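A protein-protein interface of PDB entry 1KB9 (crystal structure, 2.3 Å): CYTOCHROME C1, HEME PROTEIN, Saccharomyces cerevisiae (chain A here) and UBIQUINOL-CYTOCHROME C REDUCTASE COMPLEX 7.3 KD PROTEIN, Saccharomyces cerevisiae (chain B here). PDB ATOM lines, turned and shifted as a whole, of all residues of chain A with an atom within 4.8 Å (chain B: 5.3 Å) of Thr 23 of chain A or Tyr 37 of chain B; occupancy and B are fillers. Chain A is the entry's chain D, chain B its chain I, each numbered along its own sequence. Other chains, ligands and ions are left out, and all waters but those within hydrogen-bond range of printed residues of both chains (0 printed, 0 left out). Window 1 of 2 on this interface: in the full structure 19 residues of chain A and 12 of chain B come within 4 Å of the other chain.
The backbone carbonyl oxygen of Phe 21 of chain A sits at hydrogen-bond distance from the side-chain amide nitrogen of Asn 41 of chain B, at 2.8 Å. The side-chain amino group (NZ) of Lys 44 of chain B is in salt-bridge range of the side-chain carboxylate (OE2) of Glu 22 of chain A, 2.8 Å away. The backbone carbonyl oxygen of Ser 16 of chain A sits at hydrogen-bond distance from the side-chain amino group of Lys 44 of chain B (3.4 Å). NE2 of His 40 of chain B lies within hydrogen-bond range of OE1 of Glu 22 of chain A. The side-chain hydroxyl (OH) of Tyr 37 of chain B lies within hydrogen-bond range of the backbone carbonyl oxygen (O) of Asp 203 of chain A, 2.8 Å away. The side-chain amide oxygen of Asn 41 of chain B lies within hydrogen-bond range of the backbone NH of Thr 23 of chain A (2.7 Å). OG1 of Thr 34 of chain B is in hydrogen-bond range of NE of Arg 207 of chain A, 3.4 Å away. The backbone carbonyl oxygen (O) of Thr 23 of chain A lies close to the side-chain amino group (NZ) of Lys 44 of chain B (3.4 Å).
A ring nitrogen (NE2) of His 202 of chain A lies close to the side-chain amino group (NZ) of Lys 206 of chain A (3.3 Å). O of Glu 22 of chain A is in hydrogen-bond range of NZ of Lys 206 of chain A (3.1 Å). N of Phe 24 of chain A is in hydrogen-bond range of OD1 of Asp 203 of chain A, 2.8 Å away. A ring nitrogen (ND1) of His 202 of chain A lies within hydrogen-bond range of the side-chain carboxylate (OD1) of Asp 203 of chain A. The side-chain amino group (NZ) of Lys 44 of chain B is in hydrogen-bond range of the side-chain amide oxygen (OD1) of Asn 41 of chain B (2.8 Å). ND2 of Asn 41 of chain B is in hydrogen-bond range of O of Tyr 37 of chain B, at 3.2 Å.
Thr 23 of chain A touches four residues of chain B. Of chain A, only Phe 21, Thr 23, Asp 203, Lys 206 and Arg 207 come within 4 Å of Tyr 37 of chain B. Of the printed residues of chain B, Phe 24 of chain A touches Lys 44. Printed residues of chain B within 4 Å of Asp 25 of chain A: Lys 44. Of the printed residues of chain B, Ser 16 of chain A touches Lys 44 (3.4 Å). The nearest printed residue of chain B that does not touch Thr 23 of chain A is His 40 of chain B (6.3 Å).
Printed residues of chain B that touch a printed residue of chain A: Ile 33, Thr 34, Trp 36, Tyr 37, His 40, Asn 41, Lys 44 and Leu 45. Hydrophobic or aromatic side chains of chain B that line the printed part of chain A: Ile 33, Trp 36, Tyr 37, His 40 and Leu 45. Among the printed residues, 19 pairs touch across the chains.
Among the printed residues, merely in contact across the chains: Phe 21 of chain A with Trp 36 of chain B (3.7 Å), Phe 21 of chain A with Tyr 37 of chain B (3.7 Å), Phe 21 of chain A with His 40 of chain B (3.6 Å), Glu 22 of chain A with Asn 41 of chain B (3.6 Å), Thr 23 of chain A with Tyr 37 of chain B (3.4 Å), Thr 23 of chain A with Leu 45 of chain B (3.7 Å), Phe 24 of chain A with Lys 44 of chain B (3.5 Å), Asp 25 of chain A with Lys 44 of chain B (3.6 Å), Lys 206 of chain A with Tyr 37 of chain B (3.5 Å), Arg 207 of chain A with Tyr 37 of chain B (3.6 Å) and Leu 210 of chain A with Ile 33 of chain B (3.8 Å).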
ATOM      1  N   SER A  16      -4.946  -3.696   3.942  1.00  0.00           N
ATOM      2  CA  SER A  16      -5.959  -3.749   4.985  1.00  0.00           C
ATOM      3  C   SER A  16      -5.450  -4.441   6.257  1.00  0.00           C
ATOM      4  O   SER A  16      -5.987  -4.217   7.346  1.00  0.00           O
ATOM      5  CB  SER A  16      -7.264  -4.374   4.459  1.00  0.00           C
ATOM      6  OG  SER A  16      -7.046  -5.617   3.813  1.00  0.00           O
ATOM      7  N   HIS A  17      -4.405  -5.260   6.121  1.00  0.00           N
ATOM      8  CA  HIS A  17      -3.822  -5.935   7.280  1.00  0.00           C
ATOM      9  C   HIS A  17      -2.728  -5.130   8.000  1.00  0.00           C
ATOM     10  O   HIS A  17      -2.178  -5.593   8.999  1.00  0.00           O
ATOM     11  CB  HIS A  17      -3.336  -7.348   6.936  1.00  0.00           C
ATOM     12  CG  HIS A  17      -2.521  -7.438   5.683  1.00  0.00           C
ATOM     13  ND1 HIS A  17      -1.143  -7.471   5.695  1.00  0.00           N
ATOM     14  CD2 HIS A  17      -2.889  -7.580   4.389  1.00  0.00           C
ATOM     15  CE1 HIS A  17      -0.697  -7.635   4.462  1.00  0.00           C
ATOM     16  NE2 HIS A  17      -1.737  -7.704   3.651  1.00  0.00           N
ATOM     17  N   PHE A  21      -4.283  -3.470  15.053  1.00  0.00           N
ATOM     18  CA  PHE A  21      -5.596  -4.068  15.277  1.00  0.00           C
ATOM     19  C   PHE A  21      -6.193  -4.754  14.059  1.00  0.00           C
ATOM     20  O   PHE A  21      -7.279  -5.306  14.148  1.00  0.00           O
ATOM     21  CB  PHE A  21      -6.581  -3.003  15.763  1.00  0.00           C
ATOM     22  CG  PHE A  21      -6.047  -2.125  16.864  1.00  0.00           C
ATOM     23  CD1 PHE A  21      -6.048  -0.741  16.725  1.00  0.00           C
ATOM     24  CD2 PHE A  21      -5.554  -2.676  18.038  1.00  0.00           C
ATOM     25  CE1 PHE A  21      -5.565   0.084  17.742  1.00  0.00           C
ATOM     26  CE2 PHE A  21      -5.068  -1.860  19.062  1.00  0.00           C
ATOM     27  CZ  PHE A  21      -5.073  -0.481  18.915  1.00  0.00           C
ATOM     28  N   GLU A  22      -5.459  -4.801  12.953  1.00  0.00           N
ATOM     29  CA  GLU A  22      -5.994  -5.386  11.719  1.00  0.00           C
ATOM     30  C   GLU A  22      -5.682  -6.835  11.359  1.00  0.00           C
ATOM     31  O   GLU A  22      -4.522  -7.239  11.318  1.00  0.00           O
ATOM     32  CB  GLU A  22      -5.610  -4.501  10.533  1.00  0.00           C
ATOM     33  CG  GLU A  22      -5.832  -3.013  10.768  1.00  0.00           C
ATOM     34  CD  GLU A  22      -7.269  -2.683  11.127  1.00  0.00           C
ATOM     35  OE1 GLU A  22      -7.476  -1.805  11.989  1.00  0.00           O
ATOM     36  OE2 GLU A  22      -8.187  -3.301  10.547  1.00  0.00           O
ATOM     37  N   THR A  23      -6.727  -7.590  11.026  1.00  0.00           N
ATOM     38  CA  THR A  23      -6.577  -8.985  10.610  1.00  0.00           C
ATOM     39  C   THR A  23      -6.438  -9.006   9.094  1.00  0.00           C
ATOM     40  O   THR A  23      -6.615  -7.985   8.435  1.00  0.00           O
ATOM     41  CB  THR A  23      -7.833  -9.834  10.924  1.00  0.00           C
ATOM     42  OG1 THR A  23      -8.950  -9.341  10.163  1.00  0.00           O
ATOM     43  CG2 THR A  23      -8.163  -9.793  12.405  1.00  0.00           C
ATOM     44  N   PHE A  24      -6.121 -10.166   8.537  1.00  0.00           N
ATOM     45  CA  PHE A  24      -6.044 -10.282   7.090  1.00  0.00           C
ATOM     46  C   PHE A  24      -7.483 -10.162   6.569  1.00  0.00           C
ATOM     47  O   PHE A  24      -8.446 -10.316   7.332  1.00  0.00           O
ATOM     48  CB  PHE A  24      -5.555 -11.674   6.678  1.00  0.00           C
ATOM     49  CG  PHE A  24      -4.076 -11.868   6.766  1.00  0.00           C
ATOM     50  CD1 PHE A  24      -3.555 -13.041   7.313  1.00  0.00           C
ATOM     51  CD2 PHE A  24      -3.201 -10.928   6.246  1.00  0.00           C
ATOM     52  CE1 PHE A  24      -2.185 -13.272   7.331  1.00  0.00           C
ATOM     53  CE2 PHE A  24      -1.827 -11.154   6.261  1.00  0.00           C
ATOM     54  CZ  PHE A  24      -1.323 -12.327   6.802  1.00  0.00           C
ATOM     55  N   ASP A  25      -7.623  -9.867   5.281  1.00  0.00           N
ATOM     56  CA  ASP A  25      -8.937  -9.823   4.656  1.00  0.00           C
ATOM     57  C   ASP A  25      -9.016 -11.224   4.049  1.00  0.00           C
ATOM     58  O   ASP A  25      -8.333 -11.525   3.068  1.00  0.00           O
ATOM     59  CB  ASP A  25      -8.990  -8.765   3.555  1.00  0.00           C
ATOM     60  CG  ASP A  25     -10.367  -8.657   2.912  1.00  0.00           C
ATOM     61  OD1 ASP A  25     -11.009  -7.602   3.075  1.00  0.00           O
ATOM     62  OD2 ASP A  25     -10.807  -9.617   2.242  1.00  0.00           O
ATOM     63  N   HIS A 202      -0.679 -14.711  11.894  1.00  0.00           N
ATOM     64  CA  HIS A 202      -0.962 -13.274  11.876  1.00  0.00           C
ATOM     65  C   HIS A 202      -2.153 -12.758  12.698  1.00  0.00           C
ATOM     66  O   HIS A 202      -1.966 -11.991  13.647  1.00  0.00           O
ATOM     67  CB  HIS A 202      -1.079 -12.809  10.416  1.00  0.00           C
ATOM     68  CG  HIS A 202      -1.347 -11.344  10.249  1.00  0.00           C
ATOM     69  ND1 HIS A 202      -2.621 -10.824  10.158  1.00  0.00           N
ATOM     70  CD2 HIS A 202      -0.505 -10.292  10.128  1.00  0.00           C
ATOM     71  CE1 HIS A 202      -2.554  -9.514   9.993  1.00  0.00           C
ATOM     72  NE2 HIS A 202      -1.280  -9.165   9.971  1.00  0.00           N
ATOM     73  N   ASP A 203      -3.366 -13.193  12.354  1.00  0.00           N
ATOM     74  CA  ASP A 203      -4.577 -12.722  13.047  1.00  0.00           C
ATOM     75  C   ASP A 203      -4.599 -13.028  14.534  1.00  0.00           C
ATOM     76  O   ASP A 203      -4.935 -12.172  15.351  1.00  0.00           O
ATOM     77  CB  ASP A 203      -5.833 -13.300  12.384  1.00  0.00           C
ATOM     78  CG  ASP A 203      -5.987 -12.864  10.937  1.00  0.00           C
ATOM     79  OD1 ASP A 203      -5.260 -11.953  10.485  1.00  0.00           O
ATOM     80  OD2 ASP A 203      -6.841 -13.441  10.243  1.00  0.00           O
ATOM     81  N   LYS A 206      -1.749 -11.035  16.629  1.00  0.00           N
ATOM     82  CA  LYS A 206      -2.101  -9.663  16.981  1.00  0.00           C
ATOM     83  C   LYS A 206      -3.161  -9.581  18.071  1.00  0.00           C
ATOM     84  O   LYS A 206      -3.231  -8.599  18.808  1.00  0.00           O
ATOM     85  CB  LYS A 206      -2.583  -8.898  15.757  1.00  0.00           C
ATOM     86  CG  LYS A 206      -1.533  -8.673  14.689  1.00  0.00           C
ATOM     87  CD  LYS A 206      -2.001  -7.576  13.767  1.00  0.00           C
ATOM     88  CE  LYS A 206      -1.093  -7.419  12.588  1.00  0.00           C
ATOM     89  NZ  LYS A 206      -1.602  -6.362  11.684  1.00  0.00           N
ATOM     90  N   ARG A 207      -4.013 -10.596  18.141  1.00  0.00           N
ATOM     91  CA  ARG A 207      -5.059 -10.640  19.154  1.00  0.00           C
ATOM     92  C   ARG A 207      -4.395 -10.873  20.519  1.00  0.00           C
ATOM     93  O   ARG A 207      -4.729 -10.211  21.506  1.00  0.00           O
ATOM     94  CB  ARG A 207      -6.043 -11.767  18.832  1.00  0.00           C
ATOM     95  CG  ARG A 207      -7.357 -11.680  19.573  1.00  0.00           C
ATOM     96  CD  ARG A 207      -8.047 -13.038  19.601  1.00  0.00           C
ATOM     97  NE  ARG A 207      -8.169 -13.476  20.981  1.00  0.00           N
ATOM     98  CZ  ARG A 207      -7.728 -14.636  21.452  1.00  0.00           C
ATOM     99  NH1 ARG A 207      -7.881 -14.918  22.736  1.00  0.00           N
ATOM    100  NH2 ARG A 207      -7.169 -15.522  20.644  1.00  0.00           N
ATOM    101  N   LEU A 210      -2.545  -7.811  21.790  1.00  0.00           N
ATOM    102  CA  LEU A 210      -3.444  -6.825  22.374  1.00  0.00           C
ATOM    103  C   LEU A 210      -3.650  -7.092  23.869  1.00  0.00           C
ATOM    104  O   LEU A 210      -3.539  -6.178  24.684  1.00  0.00           O
ATOM    105  CB  LEU A 210      -4.782  -6.829  21.620  1.00  0.00           C
ATOM    106  CG  LEU A 210      -5.890  -5.861  22.070  1.00  0.00           C
ATOM    107  CD1 LEU A 210      -5.375  -4.425  22.152  1.00  0.00           C
ATOM    108  CD2 LEU A 210      -7.062  -5.963  21.099  1.00  0.00           C
ATOM    109  N   ALA B  32     -13.994 -10.167  26.313  1.00  0.00           N
ATOM    110  CA  ALA B  32     -14.077  -8.740  26.012  1.00  0.00           C
ATOM    111  C   ALA B  32     -13.160  -8.338  24.845  1.00  0.00           C
ATOM    112  O   ALA B  32     -13.577  -7.592  23.956  1.00  0.00           O
ATOM    113  CB  ALA B  32     -13.745  -7.917  27.257  1.00  0.00           C
ATOM    114  N   ILE B  33     -11.926  -8.853  24.849  1.00  0.00           N
ATOM    115  CA  ILE B  33     -10.937  -8.561  23.811  1.00  0.00           C
ATOM    116  C   ILE B  33     -11.300  -9.233  22.488  1.00  0.00           C
ATOM    117  O   ILE B  33     -11.233  -8.600  21.432  1.00  0.00           O
ATOM    118  CB  ILE B  33      -9.504  -9.007  24.240  1.00  0.00           C
ATOM    119  CG1 ILE B  33      -9.050  -8.225  25.472  1.00  0.00           C
ATOM    120  CG2 ILE B  33      -8.502  -8.798  23.105  1.00  0.00           C
ATOM    121  CD1 ILE B  33      -8.987  -6.734  25.256  1.00  0.00           C
ATOM    122  N   THR B  34     -11.663 -10.511  22.541  1.00  0.00           N
ATOM    123  CA  THR B  34     -12.042 -11.230  21.327  1.00  0.00           C
ATOM    124  C   THR B  34     -13.236 -10.543  20.656  1.00  0.00           C
ATOM    125  O   THR B  34     -13.272 -10.397  19.430  1.00  0.00           O
ATOM    126  CB  THR B  34     -12.421 -12.692  21.623  1.00  0.00           C
ATOM    127  OG1 THR B  34     -11.298 -13.379  22.192  1.00  0.00           O
ATOM    128  CG2 THR B  34     -12.850 -13.399  20.339  1.00  0.00           C
ATOM    129  N   SER B  35     -14.200 -10.106  21.465  1.00  0.00           N
ATOM    130  CA  SER B  35     -15.383  -9.427  20.941  1.00  0.00           C
ATOM    131  C   SER B  35     -15.006  -8.153  20.214  1.00  0.00           C
ATOM    132  O   SER B  35     -15.384  -7.956  19.059  1.00  0.00           O
ATOM    133  CB  SER B  35     -16.383  -9.112  22.058  1.00  0.00           C
ATOM    134  OG  SER B  35     -17.013 -10.296  22.506  1.00  0.00           O
ATOM    135  N   TRP B  36     -14.253  -7.292  20.892  1.00  0.00           N
ATOM    136  CA  TRP B  36     -13.821  -6.035  20.297  1.00  0.00           C
ATOM    137  C   TRP B  36     -13.021  -6.296  19.020  1.00  0.00           C
ATOM    138  O   TRP B  36     -13.276  -5.686  17.984  1.00  0.00           O
ATOM    139  CB  TRP B  36     -12.978  -5.236  21.293  1.00  0.00           C
ATOM    140  CG  TRP B  36     -12.557  -3.901  20.772  1.00  0.00           C
ATOM    141  CD1 TRP B  36     -13.216  -2.719  20.931  1.00  0.00           C
ATOM    142  CD2 TRP B  36     -11.410  -3.615  19.959  1.00  0.00           C
ATOM    143  NE1 TRP B  36     -12.563  -1.715  20.260  1.00  0.00           N
ATOM    144  CE2 TRP B  36     -11.450  -2.235  19.652  1.00  0.00           C
ATOM    145  CE3 TRP B  36     -10.355  -4.391  19.456  1.00  0.00           C
ATOM    146  CZ2 TRP B  36     -10.476  -1.611  18.863  1.00  0.00           C
ATOM    147  CZ3 TRP B  36      -9.387  -3.776  18.670  1.00  0.00           C
ATOM    148  CH2 TRP B  36      -9.455  -2.395  18.382  1.00  0.00           C
ATOM    149  N   TYR B  37     -12.087  -7.242  19.094  1.00  0.00           N
ATOM    150  CA  TYR B  37     -11.228  -7.588  17.965  1.00  0.00           C
ATOM    151  C   TYR B  37     -12.014  -8.043  16.737  1.00  0.00           C
ATOM    152  O   TYR B  37     -11.790  -7.535  15.636  1.00  0.00           O
ATOM    153  CB  TYR B  37     -10.222  -8.667  18.389  1.00  0.00           C
ATOM    154  CG  TYR B  37      -9.074  -8.894  17.429  1.00  0.00           C
ATOM    155  CD1 TYR B  37      -8.073  -7.928  17.258  1.00  0.00           C
ATOM    156  CD2 TYR B  37      -8.960 -10.094  16.725  1.00  0.00           C
ATOM    157  CE1 TYR B  37      -6.989  -8.155  16.412  1.00  0.00           C
ATOM    158  CE2 TYR B  37      -7.879 -10.333  15.880  1.00  0.00           C
ATOM    159  CZ  TYR B  37      -6.901  -9.361  15.727  1.00  0.00           C
ATOM    160  OH  TYR B  37      -5.847  -9.596  14.882  1.00  0.00           O
ATOM    161  N   GLU B  38     -12.917  -9.003  16.924  1.00  0.00           N
ATOM    162  CA  GLU B  38     -13.725  -9.518  15.815  1.00  0.00           C
ATOM    163  C   GLU B  38     -14.671  -8.464  15.231  1.00  0.00           C
ATOM    164  O   GLU B  38     -14.931  -8.453  14.028  1.00  0.00           O
ATOM    165  CB  GLU B  38     -14.518 -10.750  16.245  1.00  0.00           C
ATOM    166  CG  GLU B  38     -13.659 -11.949  16.550  1.00  0.00           C
ATOM    167  CD  GLU B  38     -14.459 -13.231  16.639  1.00  0.00           C
ATOM    168  OE1 GLU B  38     -13.938 -14.276  16.191  1.00  0.00           O
ATOM    169  OE2 GLU B  38     -15.603 -13.200  17.153  1.00  0.00           O
ATOM    170  N   ASN B  39     -15.180  -7.587  16.092  1.00  0.00           N
ATOM    171  CA  ASN B  39     -16.074  -6.521  15.667  1.00  0.00           C
ATOM    172  C   ASN B  39     -15.293  -5.482  14.863  1.00  0.00           C
ATOM    173  O   ASN B  39     -15.753  -5.017  13.818  1.00  0.00           O
ATOM    174  CB  ASN B  39     -16.728  -5.857  16.884  1.00  0.00           C
ATOM    175  CG  ASN B  39     -17.685  -4.746  16.493  1.00  0.00           C
ATOM    176  OD1 ASN B  39     -18.765  -5.003  15.955  1.00  0.00           O
ATOM    177  ND2 ASN B  39     -17.284  -3.501  16.738  1.00  0.00           N
ATOM    178  N   HIS B  40     -14.112  -5.119  15.356  1.00  0.00           N
ATOM    179  CA  HIS B  40     -13.260  -4.144  14.677  1.00  0.00           C
ATOM    180  C   HIS B  40     -12.890  -4.627  13.275  1.00  0.00           C
ATOM    181  O   HIS B  40     -12.679  -3.821  12.376  1.00  0.00           O
ATOM    182  CB  HIS B  40     -11.980  -3.870  15.494  1.00  0.00           C
ATOM    183  CG  HIS B  40     -11.048  -2.888  14.848  1.00  0.00           C
ATOM    184  ND1 HIS B  40     -11.106  -1.532  15.094  1.00  0.00           N
ATOM    185  CD2 HIS B  40     -10.071  -3.061  13.925  1.00  0.00           C
ATOM    186  CE1 HIS B  40     -10.211  -0.912  14.347  1.00  0.00           C
ATOM    187  NE2 HIS B  40      -9.571  -1.818  13.628  1.00  0.00           N
ATOM    188  N   ASN B  41     -12.816  -5.943  13.099  1.00  0.00           N
ATOM    189  CA  ASN B  41     -12.465  -6.532  11.808  1.00  0.00           C
ATOM    190  C   ASN B  41     -13.635  -7.152  11.048  1.00  0.00           C
ATOM    191  O   ASN B  41     -13.447  -8.040  10.213  1.00  0.00           O
ATOM    192  CB  ASN B  41     -11.349  -7.565  11.985  1.00  0.00           C
ATOM    193  CG  ASN B  41      -9.992  -6.920  12.157  1.00  0.00           C
ATOM    194  OD1 ASN B  41      -9.280  -6.688  11.179  1.00  0.00           O
ATOM    195  ND2 ASN B  41      -9.632  -6.605  13.399  1.00  0.00           N
ATOM    196  N   LYS B  44     -13.880  -8.747   7.216  1.00  0.00           N
ATOM    197  CA  LYS B  44     -12.625  -9.373   6.810  1.00  0.00           C
ATOM    198  C   LYS B  44     -12.467 -10.809   7.277  1.00  0.00           C
ATOM    199  O   LYS B  44     -11.756 -11.594   6.646  1.00  0.00           O
ATOM    200  CB  LYS B  44     -11.454  -8.531   7.307  1.00  0.00           C
ATOM    201  CG  LYS B  44     -11.342  -7.185   6.621  1.00  0.00           C
ATOM    202  CD  LYS B  44     -10.746  -6.121   7.535  1.00  0.00           C
ATOM    203  CE  LYS B  44      -9.310  -6.417   7.912  1.00  0.00           C
ATOM    204  NZ  LYS B  44      -8.768  -5.368   8.819  1.00  0.00           N
ATOM    205  N   LEU B  45     -13.140 -11.150   8.373  1.00  0.00           N
ATOM    206  CA  LEU B  45     -13.078 -12.495   8.953  1.00  0.00           C
ATOM    207  C   LEU B  45     -13.638 -13.600   8.068  1.00  0.00           C
ATOM    208  O   LEU B  45     -14.435 -13.349   7.164  1.00  0.00           O
ATOM    209  CB  LEU B  45     -13.812 -12.522  10.296  1.00  0.00           C
ATOM    210  CG  LEU B  45     -13.082 -12.133  11.585  1.00  0.00           C
ATOM    211  CD1 LEU B  45     -11.824 -11.319  11.301  1.00  0.00           C
ATOM    212  CD2 LEU B  45     -14.043 -11.377  12.495  1.00  0.00           C
